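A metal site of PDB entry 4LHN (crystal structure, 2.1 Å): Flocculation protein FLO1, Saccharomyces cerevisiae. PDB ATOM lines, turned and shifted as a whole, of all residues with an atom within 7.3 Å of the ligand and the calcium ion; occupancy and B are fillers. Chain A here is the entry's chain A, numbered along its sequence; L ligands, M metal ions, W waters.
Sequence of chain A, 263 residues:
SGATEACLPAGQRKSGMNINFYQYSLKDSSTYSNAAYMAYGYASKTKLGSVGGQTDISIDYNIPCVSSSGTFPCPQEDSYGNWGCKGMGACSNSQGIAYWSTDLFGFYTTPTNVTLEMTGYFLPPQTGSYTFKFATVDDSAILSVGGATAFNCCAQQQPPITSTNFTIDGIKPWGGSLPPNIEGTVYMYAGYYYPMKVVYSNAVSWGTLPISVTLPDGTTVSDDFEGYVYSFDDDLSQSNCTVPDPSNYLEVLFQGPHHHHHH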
ATOM      1  N   SER A  29      -2.126  24.357  -8.681  1.00  0.00           N
ATOM      2  CA  SER A  29      -1.136  25.007  -7.865  1.00  0.00           C
ATOM      3  C   SER A  29      -1.740  25.814  -6.695  1.00  0.00           C
ATOM      4  O   SER A  29      -1.074  26.649  -6.209  1.00  0.00           O
ATOM      5  CB  SER A  29      -0.307  25.919  -8.735  1.00  0.00           C
ATOM      6  OG  SER A  29      -1.178  26.934  -9.193  1.00  0.00           O
ATOM      7  N   TYR A  32      -3.130  22.444  -2.768  1.00  0.00           N
ATOM      8  CA  TYR A  32      -2.064  21.776  -2.032  1.00  0.00           C
ATOM      9  C   TYR A  32      -1.489  22.671  -0.898  1.00  0.00           C
ATOM     10  O   TYR A  32      -0.909  22.167   0.061  1.00  0.00           O
ATOM     11  CB  TYR A  32      -0.919  21.322  -3.005  1.00  0.00           C
ATOM     12  CG  TYR A  32       0.094  22.403  -3.355  1.00  0.00           C
ATOM     13  CD1 TYR A  32      -0.168  23.382  -4.305  1.00  0.00           C
ATOM     14  CD2 TYR A  32       1.313  22.457  -2.682  1.00  0.00           C
ATOM     15  CE1 TYR A  32       0.741  24.344  -4.594  1.00  0.00           C
ATOM     16  CE2 TYR A  32       2.223  23.418  -2.935  1.00  0.00           C
ATOM     17  CZ  TYR A  32       1.946  24.352  -3.900  1.00  0.00           C
ATOM     18  OH  TYR A  32       2.875  25.292  -4.135  1.00  0.00           O
ATOM     19  N   TYR A  61       9.338   9.812  -5.501  1.00  0.00           N
ATOM     20  CA  TYR A  61       8.837   9.522  -6.817  1.00  0.00           C
ATOM     21  C   TYR A  61       9.530  10.410  -7.850  1.00  0.00           C
ATOM     22  O   TYR A  61       9.630  11.600  -7.696  1.00  0.00           O
ATOM     23  CB  TYR A  61       7.313   9.790  -6.902  1.00  0.00           C
ATOM     24  CG  TYR A  61       6.819   9.680  -8.297  1.00  0.00           C
ATOM     25  CD1 TYR A  61       6.828   8.456  -8.938  1.00  0.00           C
ATOM     26  CD2 TYR A  61       6.472  10.803  -9.029  1.00  0.00           C
ATOM     27  CE1 TYR A  61       6.453   8.320 -10.248  1.00  0.00           C
ATOM     28  CE2 TYR A  61       6.021  10.697 -10.360  1.00  0.00           C
ATOM     29  CZ  TYR A  61       6.049   9.484 -10.973  1.00  0.00           C
ATOM     30  OH  TYR A  61       5.679   9.335 -12.281  1.00  0.00           O
ATOM     31  N   GLN A  76      15.528  14.088  -9.660  1.00  0.00           N
ATOM     32  CA  GLN A  76      15.215  15.463  -9.958  1.00  0.00           C
ATOM     33  C   GLN A  76      16.459  16.278 -10.082  1.00  0.00           C
ATOM     34  O   GLN A  76      16.543  17.135 -10.927  1.00  0.00           O
ATOM     35  CB  GLN A  76      14.293  16.077  -8.878  1.00  0.00           C
ATOM     36  CG  GLN A  76      13.847  17.486  -9.277  1.00  0.00           C
ATOM     37  CD  GLN A  76      12.671  18.095  -8.487  1.00  0.00           C
ATOM     38  OE1 GLN A  76      12.210  17.599  -7.441  1.00  0.00           O
ATOM     39  NE2 GLN A  76      12.179  19.201  -9.003  1.00  0.00           N
ATOM     40  N   GLN A  95       7.150  16.747 -18.871  1.00  0.00           N
ATOM     41  CA  GLN A  95       7.096  16.762 -17.434  1.00  0.00           C
ATOM     42  C   GLN A  95       5.725  17.120 -16.858  1.00  0.00           C
ATOM     43  O   GLN A  95       5.487  16.938 -15.651  1.00  0.00           O
ATOM     44  CB  GLN A  95       8.112  17.729 -16.834  1.00  0.00           C
ATOM     45  CG  GLN A  95       9.557  17.628 -17.221  1.00  0.00           C
ATOM     46  CD  GLN A  95      10.412  18.653 -16.426  1.00  0.00           C
ATOM     47  OE1 GLN A  95       9.914  19.528 -15.709  1.00  0.00           O
ATOM     48  NE2 GLN A  95      11.686  18.501 -16.514  1.00  0.00           N
ATOM     49  N   PRO A 111       1.153   8.990  -9.435  1.00  0.00           N
ATOM     50  CA  PRO A 111       1.907   9.616  -8.347  1.00  0.00           C
ATOM     51  C   PRO A 111       2.309  11.044  -8.613  1.00  0.00           C
ATOM     52  O   PRO A 111       2.684  11.735  -7.671  1.00  0.00           O
ATOM     53  CB  PRO A 111       3.129   8.718  -8.180  1.00  0.00           C
ATOM     54  CG  PRO A 111       2.920   7.542  -9.062  1.00  0.00           C
ATOM     55  CD  PRO A 111       1.984   7.988 -10.132  1.00  0.00           C
ATOM     56  N   THR A 112       2.206  11.487  -9.882  1.00  0.00           N
ATOM     57  CA  THR A 112       2.347  12.892 -10.264  1.00  0.00           C
ATOM     58  C   THR A 112       1.340  13.868  -9.658  1.00  0.00           C
ATOM     59  O   THR A 112       1.598  15.024  -9.596  1.00  0.00           O
ATOM     60  CB  THR A 112       2.154  13.054 -11.783  1.00  0.00           C
ATOM     61  OG1 THR A 112       0.989  12.340 -12.234  1.00  0.00           O
ATOM     62  CG2 THR A 112       3.359  12.520 -12.506  1.00  0.00           C
ATOM     63  N   ASP A 138       8.108  18.037  -1.576  1.00  0.00           N
ATOM     64  CA  ASP A 138       7.582  18.349  -2.889  1.00  0.00           C
ATOM     65  C   ASP A 138       6.277  17.518  -3.094  1.00  0.00           C
ATOM     66  O   ASP A 138       6.373  16.320  -3.222  1.00  0.00           O
ATOM     67  CB  ASP A 138       8.647  18.050  -3.946  1.00  0.00           C
ATOM     68  CG  ASP A 138       8.224  18.418  -5.374  1.00  0.00           C
ATOM     69  OD1 ASP A 138       7.004  18.620  -5.651  1.00  0.00           O
ATOM     70  OD2 ASP A 138       9.129  18.499  -6.230  1.00  0.00           O
ATOM     71  N   ASP A 139       5.088  18.112  -3.053  1.00  0.00           N
ATOM     72  CA  ASP A 139       4.796  19.560  -2.962  1.00  0.00           C
ATOM     73  C   ASP A 139       4.384  20.117  -1.605  1.00  0.00           C
ATOM     74  O   ASP A 139       4.694  21.272  -1.299  1.00  0.00           O
ATOM     75  CB  ASP A 139       3.676  19.876  -3.957  1.00  0.00           C
ATOM     76  CG  ASP A 139       4.160  19.874  -5.431  1.00  0.00           C
ATOM     77  OD1 ASP A 139       4.801  20.896  -5.778  1.00  0.00           O
ATOM     78  OD2 ASP A 139       3.985  18.886  -6.171  1.00  0.00           O
ATOM     79  N   SER A 140       3.638  19.351  -0.822  1.00  0.00           N
ATOM     80  CA  SER A 140       3.213  19.795   0.524  1.00  0.00           C
ATOM     81  C   SER A 140       2.909  18.605   1.405  1.00  0.00           C
ATOM     82  O   SER A 140       2.562  17.531   0.892  1.00  0.00           O
ATOM     83  CB  SER A 140       2.029  20.750   0.485  1.00  0.00           C
ATOM     84  OG  SER A 140       0.898  20.037   0.100  1.00  0.00           O
ATOM     85  N   LYS A 172       6.417  23.475  -0.684  1.00  0.00           N
ATOM     86  CA  LYS A 172       7.333  23.948  -1.725  1.00  0.00           C
ATOM     87  C   LYS A 172       6.607  25.089  -2.473  1.00  0.00           C
ATOM     88  O   LYS A 172       5.503  24.877  -3.011  1.00  0.00           O
ATOM     89  CB  LYS A 172       7.728  22.800  -2.658  1.00  0.00           C
ATOM     90  CG  LYS A 172       8.525  23.137  -3.930  1.00  0.00           C
ATOM     91  CD  LYS A 172       8.681  21.869  -4.740  1.00  0.00           C
ATOM     92  CE  LYS A 172       9.814  21.976  -5.754  1.00  0.00           C
ATOM     93  NZ  LYS A 172       9.563  23.037  -6.789  1.00  0.00           N
ATOM     94  N   PRO A 173       7.200  26.309  -2.487  1.00  0.00           N
ATOM     95  CA  PRO A 173       6.484  27.392  -3.241  1.00  0.00           C
ATOM     96  C   PRO A 173       6.465  26.984  -4.723  1.00  0.00           C
ATOM     97  O   PRO A 173       7.380  26.279  -5.194  1.00  0.00           O
ATOM     98  CB  PRO A 173       7.327  28.655  -2.999  1.00  0.00           C
ATOM     99  CG  PRO A 173       8.646  28.188  -2.384  1.00  0.00           C
ATOM    100  CD  PRO A 173       8.566  26.698  -2.053  1.00  0.00           C
ATOM    101  N   TRP A 174       5.429  27.392  -5.444  1.00  0.00           N
ATOM    102  CA  TRP A 174       5.206  26.887  -6.785  1.00  0.00           C
ATOM    103  C   TRP A 174       6.295  27.369  -7.696  1.00  0.00           C
ATOM    104  O   TRP A 174       6.425  28.524  -7.908  1.00  0.00           O
ATOM    105  CB  TRP A 174       3.895  27.399  -7.336  1.00  0.00           C
ATOM    106  CG  TRP A 174       3.535  26.726  -8.566  1.00  0.00           C
ATOM    107  CD1 TRP A 174       3.677  27.172  -9.803  1.00  0.00           C
ATOM    108  CD2 TRP A 174       3.023  25.416  -8.672  1.00  0.00           C
ATOM    109  NE1 TRP A 174       3.256  26.259 -10.695  1.00  0.00           N
ATOM    110  CE2 TRP A 174       2.863  25.147 -10.022  1.00  0.00           C
ATOM    111  CE3 TRP A 174       2.665  24.440  -7.755  1.00  0.00           C
ATOM    112  CZ2 TRP A 174       2.353  23.970 -10.472  1.00  0.00           C
ATOM    113  CZ3 TRP A 174       2.171  23.276  -8.214  1.00  0.00           C
ATOM    114  CH2 TRP A 174       2.027  23.053  -9.549  1.00  0.00           C
ATOM    115  N   GLY A 175       7.082  26.451  -8.200  1.00  0.00           N
ATOM    116  CA  GLY A 175       8.172  26.723  -9.091  1.00  0.00           C
ATOM    117  C   GLY A 175       9.482  27.000  -8.381  1.00  0.00           C
ATOM    118  O   GLY A 175      10.532  27.028  -9.004  1.00  0.00           O
ATOM    119  N   GLY A 176       9.400  27.135  -7.079  1.00  0.00           N
ATOM    120  CA  GLY A 176      10.522  27.394  -6.205  1.00  0.00           C
ATOM    121  C   GLY A 176      11.399  26.191  -5.974  1.00  0.00           C
ATOM    122  O   GLY A 176      11.063  25.102  -6.328  1.00  0.00           O
ATOM    123  N   SER A 177      12.554  26.413  -5.395  1.00  0.00           N
ATOM    124  CA  SER A 177      13.418  25.317  -5.038  1.00  0.00           C
ATOM    125  C   SER A 177      12.890  24.554  -3.807  1.00  0.00           C
ATOM    126  O   SER A 177      12.052  25.014  -3.101  1.00  0.00           O
ATOM    127  CB  SER A 177      14.847  25.799  -4.868  1.00  0.00           C
ATOM    128  OG  SER A 177      14.998  26.545  -3.703  1.00  0.00           O
ATOM    129  N   LEU A 178      13.381  23.353  -3.626  1.00  0.00           N
ATOM    130  CA  LEU A 178      12.953  22.534  -2.535  1.00  0.00           C
ATOM    131  C   LEU A 178      13.238  23.218  -1.214  1.00  0.00           C
ATOM    132  O   LEU A 178      14.256  23.839  -1.045  1.00  0.00           O
ATOM    133  CB  LEU A 178      13.642  21.195  -2.615  1.00  0.00           C
ATOM    134  CG  LEU A 178      13.276  20.365  -3.813  1.00  0.00           C
ATOM    135  CD1 LEU A 178      14.406  19.432  -4.115  1.00  0.00           C
ATOM    136  CD2 LEU A 178      11.992  19.609  -3.614  1.00  0.00           C
ATOM    137  N   TYR A 200       0.084  14.128   2.541  1.00  0.00           N
ATOM    138  CA  TYR A 200       1.083  14.493   1.540  1.00  0.00           C
ATOM    139  C   TYR A 200       0.377  14.744   0.212  1.00  0.00           C
ATOM    140  O   TYR A 200      -0.495  13.996  -0.120  1.00  0.00           O
ATOM    141  CB  TYR A 200       2.113  13.352   1.399  1.00  0.00           C
ATOM    142  CG  TYR A 200       2.920  13.512   0.141  1.00  0.00           C
ATOM    143  CD1 TYR A 200       3.956  14.439   0.053  1.00  0.00           C
ATOM    144  CD2 TYR A 200       2.646  12.791  -0.973  1.00  0.00           C
ATOM    145  CE1 TYR A 200       4.665  14.614  -1.130  1.00  0.00           C
ATOM    146  CE2 TYR A 200       3.385  12.968  -2.163  1.00  0.00           C
ATOM    147  CZ  TYR A 200       4.345  13.871  -2.233  1.00  0.00           C
ATOM    148  OH  TYR A 200       5.007  14.060  -3.405  1.00  0.00           O
ATOM    149  N   SER A 201       0.723  15.806  -0.483  1.00  0.00           N
ATOM    150  CA  SER A 201       0.265  16.075  -1.831  1.00  0.00           C
ATOM    151  C   SER A 201       1.411  16.266  -2.830  1.00  0.00           C
ATOM    152  O   SER A 201       2.377  16.923  -2.560  1.00  0.00           O
ATOM    153  CB  SER A 201      -0.661  17.282  -1.935  1.00  0.00           C
ATOM    154  OG  SER A 201      -1.752  17.243  -1.110  1.00  0.00           O
ATOM    155  N   ASN A 202       1.226  15.675  -3.991  1.00  0.00           N
ATOM    156  CA  ASN A 202       1.981  15.958  -5.177  1.00  0.00           C
ATOM    157  C   ASN A 202       1.048  16.574  -6.245  1.00  0.00           C
ATOM    158  O   ASN A 202       0.034  16.050  -6.523  1.00  0.00           O
ATOM    159  CB  ASN A 202       2.707  14.734  -5.697  1.00  0.00           C
ATOM    160  CG  ASN A 202       3.759  15.064  -6.748  1.00  0.00           C
ATOM    161  OD1 ASN A 202       4.132  16.146  -6.880  1.00  0.00           O
ATOM    162  ND2 ASN A 202       4.216  14.099  -7.452  1.00  0.00           N
ATOM    163  N   ALA A 203       1.417  17.710  -6.773  1.00  0.00           N
ATOM    164  CA  ALA A 203       0.597  18.411  -7.717  1.00  0.00           C
ATOM    165  C   ALA A 203       1.038  18.207  -9.166  1.00  0.00           C
ATOM    166  O   ALA A 203       0.253  18.253 -10.040  1.00  0.00           O
ATOM    167  CB  ALA A 203       0.557  19.864  -7.371  1.00  0.00           C
ATOM    168  N   VAL A 204       2.325  18.001  -9.382  1.00  0.00           N
ATOM    169  CA  VAL A 204       2.885  17.689 -10.690  1.00  0.00           C
ATOM    170  C   VAL A 204       4.249  17.009 -10.577  1.00  0.00           C
ATOM    171  O   VAL A 204       4.956  17.270  -9.697  1.00  0.00           O
ATOM    172  CB  VAL A 204       2.999  18.966 -11.545  1.00  0.00           C
ATOM    173  CG1 VAL A 204       4.057  19.898 -11.017  1.00  0.00           C
ATOM    174  CG2 VAL A 204       3.158  18.656 -13.011  1.00  0.00           C
ATOM    175  N   SER A 205       4.579  16.133 -11.519  1.00  0.00           N
ATOM    176  CA  SER A 205       5.944  15.601 -11.667  1.00  0.00           C
ATOM    177  C   SER A 205       6.543  15.022 -10.381  1.00  0.00           C
ATOM    178  O   SER A 205       5.942  14.184  -9.798  1.00  0.00           O
ATOM    179  CB  SER A 205       6.898  16.499 -12.482  1.00  0.00           C
ATOM    180  OG  SER A 205       7.223  17.709 -11.833  1.00  0.00           O
ATOM    181  N   TRP A 206       7.720  15.432  -9.953  1.00  0.00           N
ATOM    182  CA  TRP A 206       8.398  14.796  -8.814  1.00  0.00           C
ATOM    183  C   TRP A 206       7.655  14.882  -7.458  1.00  0.00           C
ATOM    184  O   TRP A 206       7.029  15.892  -7.159  1.00  0.00           O
ATOM    185  CB  TRP A 206       9.819  15.356  -8.663  1.00  0.00           C
ATOM    186  CG  TRP A 206      10.762  14.890  -9.724  1.00  0.00           C
ATOM    187  CD1 TRP A 206      11.496  13.734  -9.718  1.00  0.00           C
ATOM    188  CD2 TRP A 206      11.081  15.555 -10.950  1.00  0.00           C
ATOM    189  NE1 TRP A 206      12.247  13.648 -10.866  1.00  0.00           N
ATOM    190  CE2 TRP A 206      12.009  14.758 -11.636  1.00  0.00           C
ATOM    191  CE3 TRP A 206      10.658  16.759 -11.532  1.00  0.00           C
ATOM    192  CZ2 TRP A 206      12.536  15.109 -12.872  1.00  0.00           C
ATOM    193  CZ3 TRP A 206      11.185  17.110 -12.768  1.00  0.00           C
ATOM    194  CH2 TRP A 206      12.113  16.287 -13.421  1.00  0.00           C
ATOM    195  N   GLY A 207       7.757  13.825  -6.663  1.00  0.00           N
ATOM    196  CA  GLY A 207       7.240  13.818  -5.310  1.00  0.00           C
ATOM    197  C   GLY A 207       8.331  13.404  -4.335  1.00  0.00           C
ATOM    198  O   GLY A 207       9.017  12.412  -4.565  1.00  0.00           O
ATOM    199  N   THR A 208       8.497  14.156  -3.257  1.00  0.00           N
ATOM    200  CA  THR A 208       9.544  13.862  -2.289  1.00  0.00           C
ATOM    201  C   THR A 208       9.083  14.175  -0.922  1.00  0.00           C
ATOM    202  O   THR A 208       8.514  15.251  -0.718  1.00  0.00           O
ATOM    203  CB  THR A 208      10.807  14.728  -2.556  1.00  0.00           C
ATOM    204  OG1 THR A 208      11.148  14.602  -3.962  1.00  0.00           O
ATOM    205  CG2 THR A 208      11.985  14.194  -1.811  1.00  0.00           C
HETATM  206  C1  LIG L   1       9.009  21.729 -10.335  1.00  0.00           C
HETATM  207  C2  LIG L   1       9.196  20.364  -9.660  1.00  0.00           C
HETATM  208  C3  LIG L   1       7.853  19.764  -9.265  1.00  0.00           C
HETATM  209  C4  LIG L   1       6.999  20.776  -8.505  1.00  0.00           C
HETATM  210  C5  LIG L   1       6.939  22.108  -9.251  1.00  0.00           C
HETATM  211  C6  LIG L   1       6.153  23.143  -8.458  1.00  0.00           C
HETATM  212  O1  LIG L   1       8.291  21.551 -11.565  1.00  0.00           O
HETATM  213  O2  LIG L   1      10.005  20.519  -8.496  1.00  0.00           O
HETATM  214  O3  LIG L   1       8.066  18.608  -8.445  1.00  0.00           O
HETATM  215  O4  LIG L   1       5.669  20.263  -8.354  1.00  0.00           O
HETATM  216  O5  LIG L   1       8.270  22.581  -9.468  1.00  0.00           O
HETATM  217  O6  LIG L   1       6.918  23.566  -7.323  1.00  0.00           O
HETATM  218 CA    CA M   1       5.783  17.825  -7.414  1.00  0.00          CA
HETATM  219  O   HOH W   1       8.621  19.540 -13.370  1.00  0.00           O
HETATM  220  O   HOH W   2       5.153  23.485  -5.372  1.00  0.00           O
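The side-chain amide nitrogen (NE2) of Gln 76 is in hydrogen-bond range of an oxygen (O2) of the ligand, at 2.6 Å. The side-chain amino group (NZ) of Lys 172 is in hydrogen-bond range of an oxygen (O6) of the ligand (2.7 Å). The backbone NH (N) of Gly 175 sits at hydrogen-bond distance from an oxygen (O6) of the ligand (3.0 Å). O6 of the ligand is in hydrogen-bond range of O of Pro 173, 3.5 Å away.
The side-chain amide oxygen (OE1) of Gln 76 sits close to the side-chain carboxylate (OD2) of Asp 138, 3.4 Å away. The backbone carbonyl oxygen (O) of Ser 205 lies within hydrogen-bond range of the side-chain amide nitrogen (ND2) of Asn 202, at 2.9 Å. The side-chain amide nitrogen (ND2) of Asn 202 lies within hydrogen-bond range of the backbone carbonyl oxygen (O) of Pro 111, at 2.8 Å. OD2 of Asp 139 sits close to N of Ala 203, 2.9 Å away. O of Ser 201 sits at hydrogen-bond distance from N of Asp 139, 3.0 Å away. The backbone NH of Val 204 is in hydrogen-bond range of the backbone carbonyl oxygen of Thr 112 (3.1 Å). NZ of Lys 172 lies within hydrogen-bond range of O of Gly 176, at 2.6 Å. OH of Tyr 32 lies within hydrogen-bond range of O of Lys 172 (2.9 Å).
CA of Trp 174 touches O6 of the ligand, 3.8 Å away. OG of Ser 205 touches C3 of the ligand, 3.3 Å away. Hydrophobic or aromatic side chains within 4 Å of the ligand: Trp 174, Val 204 and Trp 206. Ten residues have an atom within 4 Å of the ligand: Gln 76, Asp 138, Asp 139, Lys 172, Pro 173, Trp 174, Gly 175, Val 204, Ser 205 and Trp 206.
Five residues have an atom within 4 Å of the calcium ion: Asp 138, Asp 139, Asn 202, Val 204 and Trp 206. The nearest printed residue that does not touch the calcium ion is Ser 205 (4.2 Å).
OD1 of Asp 138 is bound to the calcium ion (2.3 Å). O of Trp 206 binds the calcium ion (2.3 Å). The side-chain amide oxygen (OD1) of Asn 202 is bound to the calcium ion (2.4 Å). The side-chain carboxylate (OD2) of Asp 139 binds the calcium ion (2.4 Å). The backbone carbonyl oxygen (O) of Val 204 binds the calcium ion, 2.5 Å away. O4 of the ligand binds the calcium ion, 2.6 Å away. The calcium ion is bound by an oxygen (O3) of the ligand. The calcium ion has seven donor atoms within binding distance.
Water W2 lies within hydrogen-bond range of O6 of the ligand (2.6 Å), OD1 of Asp 139 (2.6 Å), O of Lys 172 (2.8 Å) and OH of Tyr 32 (3.2 Å). Water W1 lies within hydrogen-bond range of the side-chain amide oxygen (OE1) of Gln 95 (2.7 Å), an oxygen (O1) of the ligand (2.7 Å) and the side-chain hydroxyl (OG) of Ser 205 (2.8 Å).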
